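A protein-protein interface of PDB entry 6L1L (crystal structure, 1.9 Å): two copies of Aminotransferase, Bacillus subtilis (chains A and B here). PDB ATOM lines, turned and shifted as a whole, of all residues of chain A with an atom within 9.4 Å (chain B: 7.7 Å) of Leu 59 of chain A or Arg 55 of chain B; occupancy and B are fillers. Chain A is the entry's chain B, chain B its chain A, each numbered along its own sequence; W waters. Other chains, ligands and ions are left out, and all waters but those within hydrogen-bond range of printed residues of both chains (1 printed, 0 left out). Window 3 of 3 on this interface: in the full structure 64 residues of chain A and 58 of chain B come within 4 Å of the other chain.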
ATOM      1  N   VAL A  51      -6.223  34.562  22.776  1.00  0.00           N
ATOM      2  CA  VAL A  51      -5.240  33.502  22.937  1.00  0.00           C
ATOM      3  C   VAL A  51      -5.813  32.349  23.794  1.00  0.00           C
ATOM      4  O   VAL A  51      -5.631  31.156  23.493  1.00  0.00           O
ATOM      5  CB  VAL A  51      -3.945  34.008  23.592  1.00  0.00           C
ATOM      6  CG1 VAL A  51      -3.011  32.861  23.853  1.00  0.00           C
ATOM      7  CG2 VAL A  51      -3.221  34.997  22.691  1.00  0.00           C
ATOM      8  N   GLU A  52      -6.471  32.700  24.882  1.00  0.00           N
ATOM      9  CA  GLU A  52      -7.011  31.620  25.749  1.00  0.00           C
ATOM     10  C   GLU A  52      -8.174  30.875  25.099  1.00  0.00           C
ATOM     11  O   GLU A  52      -8.326  29.664  25.281  1.00  0.00           O
ATOM     12  CB  GLU A  52      -7.371  32.155  27.129  1.00  0.00           C
ATOM     13  CG  GLU A  52      -6.180  32.795  27.872  1.00  0.00           C
ATOM     14  CD  GLU A  52      -4.862  32.012  27.781  1.00  0.00           C
ATOM     15  OE1 GLU A  52      -4.891  30.776  27.956  1.00  0.00           O
ATOM     16  OE2 GLU A  52      -3.783  32.627  27.522  1.00  0.00           O
ATOM     17  N   ALA A  53      -8.965  31.586  24.297  1.00  0.00           N
ATOM     18  CA  ALA A  53     -10.043  30.954  23.510  1.00  0.00           C
ATOM     19  C   ALA A  53      -9.485  29.833  22.613  1.00  0.00           C
ATOM     20  O   ALA A  53     -10.027  28.746  22.585  1.00  0.00           O
ATOM     21  CB  ALA A  53     -10.746  31.979  22.646  1.00  0.00           C
ATOM     22  N   LEU A  54      -8.409  30.112  21.896  1.00  0.00           N
ATOM     23  CA  LEU A  54      -7.717  29.074  21.082  1.00  0.00           C
ATOM     24  C   LEU A  54      -7.201  27.915  21.940  1.00  0.00           C
ATOM     25  O   LEU A  54      -7.300  26.747  21.574  1.00  0.00           O
ATOM     26  CB  LEU A  54      -6.568  29.696  20.259  1.00  0.00           C
ATOM     27  CG  LEU A  54      -5.543  28.753  19.601  1.00  0.00           C
ATOM     28  CD1 LEU A  54      -6.152  27.769  18.595  1.00  0.00           C
ATOM     29  CD2 LEU A  54      -4.428  29.535  18.905  1.00  0.00           C
ATOM     30  N   ARG A  55      -6.610  28.257  23.071  1.00  0.00           N
ATOM     31  CA  ARG A  55      -5.987  27.281  23.913  1.00  0.00           C
ATOM     32  C   ARG A  55      -6.999  26.272  24.468  1.00  0.00           C
ATOM     33  O   ARG A  55      -6.781  25.072  24.393  1.00  0.00           O
ATOM     34  CB  ARG A  55      -5.210  27.958  25.020  1.00  0.00           C
ATOM     35  CG  ARG A  55      -3.937  28.608  24.496  1.00  0.00           C
ATOM     36  CD  ARG A  55      -3.085  29.169  25.585  1.00  0.00           C
ATOM     37  NE  ARG A  55      -2.403  28.099  26.285  1.00  0.00           N
ATOM     38  CZ  ARG A  55      -2.639  27.758  27.542  1.00  0.00           C
ATOM     39  NH1 ARG A  55      -3.538  28.411  28.256  1.00  0.00           N
ATOM     40  NH2 ARG A  55      -1.985  26.746  28.073  1.00  0.00           N
ATOM     41  N   GLU A  56      -8.137  26.762  24.913  1.00  0.00           N
ATOM     42  CA  GLU A  56      -9.191  25.894  25.445  1.00  0.00           C
ATOM     43  C   GLU A  56      -9.847  25.091  24.326  1.00  0.00           C
ATOM     44  O   GLU A  56      -9.986  23.867  24.420  1.00  0.00           O
ATOM     45  CB  GLU A  56     -10.212  26.739  26.199  1.00  0.00           C
ATOM     46  N   ALA A  57     -10.170  25.780  23.218  1.00  0.00           N
ATOM     47  CA  ALA A  57     -10.791  25.141  22.051  1.00  0.00           C
ATOM     48  C   ALA A  57      -9.986  23.999  21.457  1.00  0.00           C
ATOM     49  O   ALA A  57     -10.558  23.042  20.995  1.00  0.00           O
ATOM     50  CB  ALA A  57     -11.091  26.168  20.996  1.00  0.00           C
ATOM     51  N   SER A  58      -8.651  24.093  21.458  1.00  0.00           N
ATOM     52  CA  SER A  58      -7.823  23.032  20.869  1.00  0.00           C
ATOM     53  C   SER A  58      -7.949  21.679  21.602  1.00  0.00           C
ATOM     54  O   SER A  58      -7.652  20.625  21.051  1.00  0.00           O
ATOM     55  CB  SER A  58      -6.353  23.474  20.825  1.00  0.00           C
ATOM     56  OG  SER A  58      -5.777  23.456  22.137  1.00  0.00           O
ATOM     57  N   LEU A  59      -8.373  21.724  22.853  1.00  0.00           N
ATOM     58  CA  LEU A  59      -8.671  20.519  23.624  1.00  0.00           C
ATOM     59  C   LEU A  59      -9.947  19.792  23.208  1.00  0.00           C
ATOM     60  O   LEU A  59     -10.142  18.604  23.576  1.00  0.00           O
ATOM     61  CB  LEU A  59      -8.740  20.884  25.104  1.00  0.00           C
ATOM     62  CG  LEU A  59      -7.456  21.382  25.717  1.00  0.00           C
ATOM     63  CD1 LEU A  59      -7.705  22.072  27.048  1.00  0.00           C
ATOM     64  CD2 LEU A  59      -6.495  20.222  25.910  1.00  0.00           C
ATOM     65  N   ASN A  60     -10.784  20.450  22.404  1.00  0.00           N
ATOM     66  CA  ASN A  60     -12.058  19.885  21.948  1.00  0.00           C
ATOM     67  C   ASN A  60     -11.892  18.977  20.720  1.00  0.00           C
ATOM     68  O   ASN A  60     -11.827  19.499  19.582  1.00  0.00           O
ATOM     69  CB  ASN A  60     -13.072  20.989  21.675  1.00  0.00           C
ATOM     70  CG  ASN A  60     -14.442  20.447  21.207  1.00  0.00           C
ATOM     71  OD1 ASN A  60     -14.602  19.258  20.947  1.00  0.00           O
ATOM     72  ND2 ASN A  60     -15.420  21.327  21.088  1.00  0.00           N
ATOM     73  N   PRO A  61     -11.945  17.624  20.922  1.00  0.00           N
ATOM     74  CA  PRO A  61     -11.654  16.677  19.858  1.00  0.00           C
ATOM     75  C   PRO A  61     -12.579  16.792  18.635  1.00  0.00           C
ATOM     76  O   PRO A  61     -12.158  16.414  17.539  1.00  0.00           O
ATOM     77  CB  PRO A  61     -11.704  15.293  20.547  1.00  0.00           C
ATOM     78  CG  PRO A  61     -12.532  15.499  21.732  1.00  0.00           C
ATOM     79  CD  PRO A  61     -12.398  16.937  22.153  1.00  0.00           C
ATOM     80  N   SER A  62     -13.773  17.387  18.796  1.00  0.00           N
ATOM     81  CA  SER A  62     -14.649  17.694  17.681  1.00  0.00           C
ATOM     82  C   SER A  62     -13.920  18.512  16.610  1.00  0.00           C
ATOM     83  O   SER A  62     -14.253  18.406  15.422  1.00  0.00           O
ATOM     84  CB  SER A  62     -15.898  18.484  18.155  1.00  0.00           C
ATOM     85  OG  SER A  62     -16.687  17.717  19.042  1.00  0.00           O
ATOM     86  N   PHE A  63     -12.957  19.347  17.033  1.00  0.00           N
ATOM     87  CA  PHE A  63     -12.187  20.146  16.098  1.00  0.00           C
ATOM     88  C   PHE A  63     -10.948  19.410  15.570  1.00  0.00           C
ATOM     89  O   PHE A  63     -10.211  19.966  14.730  1.00  0.00           O
ATOM     90  CB  PHE A  63     -11.753  21.478  16.736  1.00  0.00           C
ATOM     91  CG  PHE A  63     -12.882  22.411  17.118  1.00  0.00           C
ATOM     92  CD1 PHE A  63     -14.002  22.567  16.332  1.00  0.00           C
ATOM     93  CD2 PHE A  63     -12.790  23.163  18.281  1.00  0.00           C
ATOM     94  CE1 PHE A  63     -15.013  23.467  16.670  1.00  0.00           C
ATOM     95  CE2 PHE A  63     -13.803  24.062  18.634  1.00  0.00           C
ATOM     96  CZ  PHE A  63     -14.909  24.215  17.811  1.00  0.00           C
ATOM     97  N   HIS A  64     -10.698  18.181  15.977  1.00  0.00           N
ATOM     98  CA  HIS A  64      -9.498  17.492  15.475  1.00  0.00           C
ATOM     99  C   HIS A  64      -9.798  16.862  14.113  1.00  0.00           C
ATOM    100  O   HIS A  64      -8.892  16.649  13.293  1.00  0.00           O
ATOM    101  CB  HIS A  64      -8.938  16.491  16.445  1.00  0.00           C
ATOM    102  CG  HIS A  64      -8.561  17.064  17.776  1.00  0.00           C
ATOM    103  ND1 HIS A  64      -8.099  16.275  18.816  1.00  0.00           N
ATOM    104  CD2 HIS A  64      -8.553  18.327  18.247  1.00  0.00           C
ATOM    105  CE1 HIS A  64      -7.861  17.019  19.877  1.00  0.00           C
ATOM    106  NE2 HIS A  64      -8.114  18.271  19.562  1.00  0.00           N
ATOM    107  N   TRP A 246      -2.326  34.816  12.416  1.00  0.00           N
ATOM    108  CA  TRP A 246      -3.357  33.765  12.603  1.00  0.00           C
ATOM    109  C   TRP A 246      -4.051  33.383  11.283  1.00  0.00           C
ATOM    110  O   TRP A 246      -4.566  32.284  11.157  1.00  0.00           O
ATOM    111  CB  TRP A 246      -4.429  34.258  13.553  1.00  0.00           C
ATOM    112  CG  TRP A 246      -3.940  34.459  14.975  1.00  0.00           C
ATOM    113  CD1 TRP A 246      -2.897  35.264  15.389  1.00  0.00           C
ATOM    114  CD2 TRP A 246      -4.477  33.867  16.153  1.00  0.00           C
ATOM    115  NE1 TRP A 246      -2.776  35.222  16.750  1.00  0.00           N
ATOM    116  CE2 TRP A 246      -3.730  34.373  17.249  1.00  0.00           C
ATOM    117  CE3 TRP A 246      -5.532  32.962  16.404  1.00  0.00           C
ATOM    118  CZ2 TRP A 246      -4.005  34.019  18.569  1.00  0.00           C
ATOM    119  CZ3 TRP A 246      -5.793  32.594  17.712  1.00  0.00           C
ATOM    120  CH2 TRP A 246      -5.018  33.122  18.794  1.00  0.00           C
ATOM    121  N   PHE A 273      -9.049  25.304  11.047  1.00  0.00           N
ATOM    122  CA  PHE A 273      -9.099  24.652  12.361  1.00  0.00           C
ATOM    123  C   PHE A 273     -10.130  25.246  13.247  1.00  0.00           C
ATOM    124  O   PHE A 273     -10.211  26.446  13.386  1.00  0.00           O
ATOM    125  CB  PHE A 273      -7.742  24.758  13.061  1.00  0.00           C
ATOM    126  CG  PHE A 273      -7.653  24.043  14.370  1.00  0.00           C
ATOM    127  CD1 PHE A 273      -7.978  22.674  14.472  1.00  0.00           C
ATOM    128  CD2 PHE A 273      -7.187  24.690  15.490  1.00  0.00           C
ATOM    129  CE1 PHE A 273      -7.871  22.016  15.667  1.00  0.00           C
ATOM    130  CE2 PHE A 273      -7.057  24.019  16.697  1.00  0.00           C
ATOM    131  CZ  PHE A 273      -7.406  22.682  16.785  1.00  0.00           C
ATOM    132  N   GLY A 274     -10.895  24.398  13.900  1.00  0.00           N
ATOM    133  CA  GLY A 274     -11.980  24.894  14.700  1.00  0.00           C
ATOM    134  C   GLY A 274     -11.509  25.718  15.883  1.00  0.00           C
ATOM    135  O   GLY A 274     -12.179  26.637  16.290  1.00  0.00           O
ATOM    136  N   GLY A 275     -10.336  25.404  16.423  1.00  0.00           N
ATOM    137  CA  GLY A 275      -9.729  26.260  17.435  1.00  0.00           C
ATOM    138  C   GLY A 275      -9.544  27.699  17.028  1.00  0.00           C
ATOM    139  O   GLY A 275      -9.761  28.577  17.818  1.00  0.00           O
ATOM    140  N   GLN A 278     -13.138  29.472  16.897  1.00  0.00           N
ATOM    141  CA  GLN A 278     -13.535  29.887  18.261  1.00  0.00           C
ATOM    142  C   GLN A 278     -12.765  31.097  18.784  1.00  0.00           C
ATOM    143  O   GLN A 278     -13.336  31.996  19.359  1.00  0.00           O
ATOM    144  CB  GLN A 278     -13.425  28.722  19.234  1.00  0.00           C
ATOM    145  CG  GLN A 278     -13.943  29.002  20.637  1.00  0.00           C
ATOM    146  CD  GLN A 278     -15.403  29.387  20.665  1.00  0.00           C
ATOM    147  OE1 GLN A 278     -16.278  28.574  20.323  1.00  0.00           O
ATOM    148  NE2 GLN A 278     -15.692  30.638  21.083  1.00  0.00           N
ATOM    149  N   PRO B  45      -8.864  11.078  18.428  1.00  0.00           N
ATOM    150  CA  PRO B  45      -8.376  12.440  18.577  1.00  0.00           C
ATOM    151  C   PRO B  45      -6.889  12.613  18.153  1.00  0.00           C
ATOM    152  O   PRO B  45      -6.100  11.670  18.065  1.00  0.00           O
ATOM    153  CB  PRO B  45      -8.547  12.702  20.104  1.00  0.00           C
ATOM    154  CG  PRO B  45      -8.373  11.353  20.709  1.00  0.00           C
ATOM    155  CD  PRO B  45      -9.004  10.396  19.740  1.00  0.00           C
ATOM    156  N   PRO B  48      -2.238  13.930  22.255  1.00  0.00           N
ATOM    157  CA  PRO B  48      -2.064  14.957  23.246  1.00  0.00           C
ATOM    158  C   PRO B  48      -0.779  15.819  23.119  1.00  0.00           C
ATOM    159  O   PRO B  48      -0.798  16.981  23.457  1.00  0.00           O
ATOM    160  CB  PRO B  48      -1.963  14.141  24.560  1.00  0.00           C
ATOM    161  CG  PRO B  48      -2.718  12.898  24.287  1.00  0.00           C
ATOM    162  CD  PRO B  48      -2.534  12.615  22.857  1.00  0.00           C
ATOM    163  N   HIS B  49       0.316  15.231  22.690  1.00  0.00           N
ATOM    164  CA  HIS B  49       1.573  15.998  22.571  1.00  0.00           C
ATOM    165  C   HIS B  49       1.561  17.023  21.438  1.00  0.00           C
ATOM    166  O   HIS B  49       2.317  17.976  21.462  1.00  0.00           O
ATOM    167  CB  HIS B  49       2.776  15.084  22.441  1.00  0.00           C
ATOM    168  CG  HIS B  49       2.854  14.305  21.161  1.00  0.00           C
ATOM    169  ND1 HIS B  49       2.015  13.246  20.870  1.00  0.00           N
ATOM    170  CD2 HIS B  49       3.723  14.383  20.123  1.00  0.00           C
ATOM    171  CE1 HIS B  49       2.375  12.695  19.726  1.00  0.00           C
ATOM    172  NE2 HIS B  49       3.399  13.373  19.245  1.00  0.00           N
ATOM    173  N   ILE B  50       0.733  16.774  20.443  1.00  0.00           N
ATOM    174  CA  ILE B  50       0.573  17.689  19.328  1.00  0.00           C
ATOM    175  C   ILE B  50      -0.326  18.868  19.794  1.00  0.00           C
ATOM    176  O   ILE B  50      -0.052  20.026  19.542  1.00  0.00           O
ATOM    177  CB  ILE B  50       0.005  16.916  18.096  1.00  0.00           C
ATOM    178  CG1 ILE B  50       0.989  15.826  17.660  1.00  0.00           C
ATOM    179  CG2 ILE B  50      -0.231  17.861  16.970  1.00  0.00           C
ATOM    180  CD1 ILE B  50       0.461  14.809  16.673  1.00  0.00           C
ATOM    181  N   VAL B  51      -1.410  18.541  20.471  1.00  0.00           N
ATOM    182  CA  VAL B  51      -2.294  19.530  21.072  1.00  0.00           C
ATOM    183  C   VAL B  51      -1.537  20.410  22.062  1.00  0.00           C
ATOM    184  O   VAL B  51      -1.768  21.639  22.082  1.00  0.00           O
ATOM    185  CB  VAL B  51      -3.514  18.874  21.806  1.00  0.00           C
ATOM    186  CG1 VAL B  51      -4.431  19.942  22.434  1.00  0.00           C
ATOM    187  CG2 VAL B  51      -4.311  17.957  20.891  1.00  0.00           C
ATOM    188  N   GLU B  52      -0.657  19.791  22.882  1.00  0.00           N
ATOM    189  CA  GLU B  52       0.114  20.585  23.875  1.00  0.00           C
ATOM    190  C   GLU B  52       1.056  21.545  23.177  1.00  0.00           C
ATOM    191  O   GLU B  52       1.176  22.712  23.575  1.00  0.00           O
ATOM    192  CB  GLU B  52       0.928  19.714  24.841  1.00  0.00           C
ATOM    193  N   ALA B  53       1.679  21.074  22.100  1.00  0.00           N
ATOM    194  CA  ALA B  53       2.595  21.944  21.336  1.00  0.00           C
ATOM    195  C   ALA B  53       1.857  23.193  20.792  1.00  0.00           C
ATOM    196  O   ALA B  53       2.391  24.315  20.858  1.00  0.00           O
ATOM    197  CB  ALA B  53       3.215  21.153  20.221  1.00  0.00           C
ATOM    198  N   LEU B  54       0.655  23.005  20.237  1.00  0.00           N
ATOM    199  CA  LEU B  54      -0.167  24.137  19.786  1.00  0.00           C
ATOM    200  C   LEU B  54      -0.506  25.062  20.961  1.00  0.00           C
ATOM    201  O   LEU B  54      -0.357  26.293  20.875  1.00  0.00           O
ATOM    202  CB  LEU B  54      -1.469  23.706  19.126  1.00  0.00           C
ATOM    203  CG  LEU B  54      -2.437  24.845  18.800  1.00  0.00           C
ATOM    204  CD1 LEU B  54      -1.860  25.836  17.761  1.00  0.00           C
ATOM    205  CD2 LEU B  54      -3.767  24.306  18.293  1.00  0.00           C
ATOM    206  N   ARG B  55      -0.961  24.460  22.065  1.00  0.00           N
ATOM    207  CA  ARG B  55      -1.323  25.243  23.248  1.00  0.00           C
ATOM    208  C   ARG B  55      -0.157  26.066  23.793  1.00  0.00           C
ATOM    209  O   ARG B  55      -0.350  27.195  24.159  1.00  0.00           O
ATOM    210  CB  ARG B  55      -1.902  24.371  24.346  1.00  0.00           C
ATOM    211  CG  ARG B  55      -3.307  23.910  24.056  1.00  0.00           C
ATOM    212  CD  ARG B  55      -3.742  22.787  24.984  1.00  0.00           C
ATOM    213  NE  ARG B  55      -3.378  23.124  26.365  1.00  0.00           N
ATOM    214  CZ  ARG B  55      -4.091  23.882  27.163  1.00  0.00           C
ATOM    215  NH1 ARG B  55      -5.264  24.368  26.765  1.00  0.00           N
ATOM    216  NH2 ARG B  55      -3.651  24.131  28.372  1.00  0.00           N
ATOM    217  N   GLU B  56       1.035  25.491  23.839  1.00  0.00           N
ATOM    218  CA  GLU B  56       2.205  26.190  24.295  1.00  0.00           C
ATOM    219  C   GLU B  56       2.641  27.278  23.326  1.00  0.00           C
ATOM    220  O   GLU B  56       2.855  28.425  23.739  1.00  0.00           O
ATOM    221  CB  GLU B  56       3.355  25.207  24.519  1.00  0.00           C
ATOM    222  CG  GLU B  56       4.411  25.712  25.480  1.00  0.00           C
ATOM    223  CD  GLU B  56       5.372  24.607  25.898  1.00  0.00           C
ATOM    224  OE1 GLU B  56       4.921  23.449  26.082  1.00  0.00           O
ATOM    225  OE2 GLU B  56       6.588  24.870  26.045  1.00  0.00           O
ATOM    226  N   ALA B  57       2.724  26.937  22.038  1.00  0.00           N
ATOM    227  CA  ALA B  57       3.208  27.898  21.029  1.00  0.00           C
ATOM    228  C   ALA B  57       2.366  29.126  20.924  1.00  0.00           C
ATOM    229  O   ALA B  57       2.889  30.214  20.675  1.00  0.00           O
ATOM    230  CB  ALA B  57       3.318  27.261  19.691  1.00  0.00           C
ATOM    231  N   SER B  58       1.067  28.981  21.157  1.00  0.00           N
ATOM    232  CA  SER B  58       0.138  30.078  21.006  1.00  0.00           C
ATOM    233  C   SER B  58       0.369  31.255  21.949  1.00  0.00           C
ATOM    234  O   SER B  58      -0.060  32.361  21.672  1.00  0.00           O
ATOM    235  CB  SER B  58      -1.297  29.551  21.184  1.00  0.00           C
ATOM    236  OG  SER B  58      -1.539  29.368  22.582  1.00  0.00           O
ATOM    237  N   LEU B  59       1.040  31.006  23.068  1.00  0.00           N
ATOM    238  CA  LEU B  59       1.412  32.040  24.019  1.00  0.00           C
ATOM    239  C   LEU B  59       2.557  32.943  23.548  1.00  0.00           C
ATOM    240  O   LEU B  59       2.749  34.026  24.109  1.00  0.00           O
ATOM    241  CB  LEU B  59       1.839  31.395  25.337  1.00  0.00           C
ATOM    242  CG  LEU B  59       0.749  30.533  25.975  1.00  0.00           C
ATOM    243  CD1 LEU B  59       1.284  29.875  27.237  1.00  0.00           C
ATOM    244  CD2 LEU B  59      -0.462  31.349  26.291  1.00  0.00           C
ATOM    245  N   ASN B  60       3.290  32.489  22.533  1.00  0.00           N
ATOM    246  CA  ASN B  60       4.492  33.154  22.036  1.00  0.00           C
ATOM    247  C   ASN B  60       4.129  34.262  21.049  1.00  0.00           C
ATOM    248  O   ASN B  60       3.819  33.977  19.890  1.00  0.00           O
ATOM    249  CB  ASN B  60       5.407  32.132  21.366  1.00  0.00           C
ATOM    250  CG  ASN B  60       6.686  32.752  20.825  1.00  0.00           C
ATOM    251  OD1 ASN B  60       6.954  33.940  21.032  1.00  0.00           O
ATOM    252  ND2 ASN B  60       7.465  31.951  20.096  1.00  0.00           N
ATOM    253  N   TRP B 246      -7.054  20.321  11.202  1.00  0.00           N
ATOM    254  CA  TRP B 246      -6.062  21.279  11.445  1.00  0.00           C
ATOM    255  C   TRP B 246      -5.626  21.932  10.124  1.00  0.00           C
ATOM    256  O   TRP B 246      -5.148  23.066  10.148  1.00  0.00           O
ATOM    257  CB  TRP B 246      -4.881  20.667  12.127  1.00  0.00           C
ATOM    258  CG  TRP B 246      -5.150  20.157  13.506  1.00  0.00           C
ATOM    259  CD1 TRP B 246      -6.048  19.233  13.882  1.00  0.00           C
ATOM    260  CD2 TRP B 246      -4.397  20.493  14.682  1.00  0.00           C
ATOM    261  NE1 TRP B 246      -5.962  19.006  15.263  1.00  0.00           N
ATOM    262  CE2 TRP B 246      -4.940  19.766  15.755  1.00  0.00           C
ATOM    263  CE3 TRP B 246      -3.317  21.334  14.924  1.00  0.00           C
ATOM    264  CZ2 TRP B 246      -4.448  19.874  17.052  1.00  0.00           C
ATOM    265  CZ3 TRP B 246      -2.839  21.450  16.234  1.00  0.00           C
ATOM    266  CH2 TRP B 246      -3.414  20.724  17.275  1.00  0.00           C
ATOM    267  N   GLY B 275       1.700  28.693  15.723  1.00  0.00           N
ATOM    268  CA  GLY B 275       1.219  27.617  16.628  1.00  0.00           C
ATOM    269  C   GLY B 275       0.945  26.297  15.923  1.00  0.00           C
ATOM    270  O   GLY B 275       1.348  25.269  16.371  1.00  0.00           O
ATOM    271  N   LEU B 276       0.266  26.358  14.772  1.00  0.00           N
ATOM    272  CA  LEU B 276       0.088  25.194  13.946  1.00  0.00           C
ATOM    273  C   LEU B 276       1.375  24.607  13.481  1.00  0.00           C
ATOM    274  O   LEU B 276       1.515  23.368  13.421  1.00  0.00           O
ATOM    275  CB  LEU B 276      -0.777  25.504  12.699  1.00  0.00           C
ATOM    276  CG  LEU B 276      -2.212  26.006  12.968  1.00  0.00           C
ATOM    277  CD1 LEU B 276      -2.904  26.133  11.597  1.00  0.00           C
ATOM    278  CD2 LEU B 276      -2.998  25.077  13.877  1.00  0.00           C
ATOM    279  N   GLN B 278       4.282  24.782  14.874  1.00  0.00           N
ATOM    280  CA  GLN B 278       4.937  24.154  16.014  1.00  0.00           C
ATOM    281  C   GLN B 278       4.294  22.794  16.241  1.00  0.00           C
ATOM    282  O   GLN B 278       4.972  21.841  16.429  1.00  0.00           O
ATOM    283  CB  GLN B 278       4.800  25.003  17.260  1.00  0.00           C
ATOM    284  CG  GLN B 278       5.782  24.717  18.357  1.00  0.00           C
ATOM    285  CD  GLN B 278       6.971  25.664  18.288  1.00  0.00           C
ATOM    286  OE1 GLN B 278       6.923  26.758  18.844  1.00  0.00           O
ATOM    287  NE2 GLN B 278       8.034  25.256  17.603  1.00  0.00           N
ATOM    288  N   ALA B 279       2.968  22.736  16.196  1.00  0.00           N
ATOM    289  CA  ALA B 279       2.237  21.495  16.404  1.00  0.00           C
ATOM    290  C   ALA B 279       2.622  20.462  15.362  1.00  0.00           C
ATOM    291  O   ALA B 279       2.835  19.306  15.689  1.00  0.00           O
ATOM    292  CB  ALA B 279       0.752  21.747  16.383  1.00  0.00           C
HETATM  293  O   HOH W   1      -6.292  25.732  10.031  1.00  0.00           O
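OG of Ser 58 of chain B is in hydrogen-bond range of O of Arg 55 of chain B, at 2.9 Å.
The side-chain hydroxyl (OG) of Ser 58 of chain A is in hydrogen-bond range of the backbone carbonyl oxygen (O) of Arg 55 of chain A (3.0 Å).
A ring nitrogen (NE2) of His 64 of chain A lies within hydrogen-bond range of the backbone carbonyl oxygen (O) of Ser 58 of chain A (2.8 Å).
The guanidinium group (NH1) of Arg 55 of chain A lies within salt-bridge range of the side-chain carboxylate (OE1) of Glu 52 of chain A (2.7 Å).
Val 51 of chain A touches Ser 58 of chain B, and with the chains exchanged Ser 58 of chain A touches Val 51 of chain B.
Leu 54 of chain A touches Ser 58 of chain B, and with the chains exchanged Ser 58 of chain A touches Leu 54 of chain B.
Arg 55 of chain A touches Ser 58 of chain B, and with the chains exchanged Ser 58 of chain A touches Arg 55 of chain B.
Arg 55 of chain A touches Leu 59 of chain B, and with the chains exchanged Leu 59 of chain A touches Arg 55 of chain B.
Of the 16 pairs that touch across the chains among the printed residues, 9 have their exchanged pair printed and touching as well.
Printed residues of chain A that touch a printed residue of chain B: Val 51, Glu 52, Leu 54, Arg 55, Ser 58, Leu 59, His 64 and Phe 273.
Printed residues of chain B that touch a printed residue of chain A: Pro 45, Val 51, Leu 54, Arg 55, Ser 58, Leu 59 and Trp 246.
Hydrophobic or aromatic side chains of chain B that line the printed part of chain A: Pro 45, Val 51, Leu 54, Leu 59 and Trp 246.
Among the printed residues, 16 pairs touch across the chains.
Among the printed residues, no Asp or Glu carboxylate lies within 4 Å of a Lys or Arg side-chain nitrogen of the other chain.
Val 51 of chain A touches Ser 58 of chain B.
CD2 of Leu 59 of chain B touches CG1 of Val 51 of chain A, 3.8 Å away.
Leu 59 of chain B touches Glu 52 of chain A.
Ser 58 of chain B touches Arg 55 of chain A.
Arg 55 of chain A touches Leu 59 of chain B.
CG1 of Val 51 of chain B touches O of Ser 58 of chain A (3.6 Å).
OG of Ser 58 of chain A touches CG of Arg 55 of chain B (3.2 Å).
Leu 59 of chain A touches Arg 55 of chain B.
ND1 of His 64 of chain A touches CB of Pro 45 of chain B, at 3.8 Å.
CE1 of Phe 273 of chain A touches NE1 of Trp 246 of chain B (3.6 Å).
Leu 59 of chain A touches one residue of chain B.
Arg 55 of chain B touches three residues of chain A.
Of chain B, only Val 51 (3.6 Å), Leu 54 (3.7 Å) and Arg 55 (3.2 Å) come within 4 Å of Ser 58 of chain A.
Leu 54 of chain B touches just these residues of chain A: Ser 58 and Phe 273.
Of the printed residues of chain B, Phe 273 of chain A touches Leu 54 (3.7 Å) and Trp 246 (3.6 Å).
Printed residues of chain B within 4 Å of His 64 of chain A: Pro 45 (3.8 Å), Val 51 (3.8 Å) and Trp 246 (3.9 Å).
Of the printed residues of chain A, Pro 45 of chain B touches His 64 (3.8 Å).
Printed residues of chain A within 4 Å of Ser 58 of chain B: Val 51 (3.7 Å), Leu 54 (3.9 Å) and Arg 55 (3.2 Å).
Of the printed residues of chain B, Leu 54 of chain A touches Ser 58.
His 49 of chain B touches none of the printed residues of chain A.
Pro 48 of chain B touches none of the printed residues of chain A.
The nearest residue of chain B that does not touch Leu 59 of chain A is Val 51 of chain B (4.1 Å).
The nearest printed residue of chain A that does not touch Leu 59 of chain B is Leu 54 of chain A (7.0 Å).
Water W1 lies within hydrogen-bond range of the backbone carbonyl oxygen (O) of Trp 246 of chain B (2.9 Å) and the backbone NH (N) of Phe 273 of chain A (3.0 Å).
The backbone carbonyl oxygen (O) of Arg 55 of chain A lies within hydrogen-bond range of the guanidinium group (NH1) of Arg 55 of chain B, 2.9 Å away.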
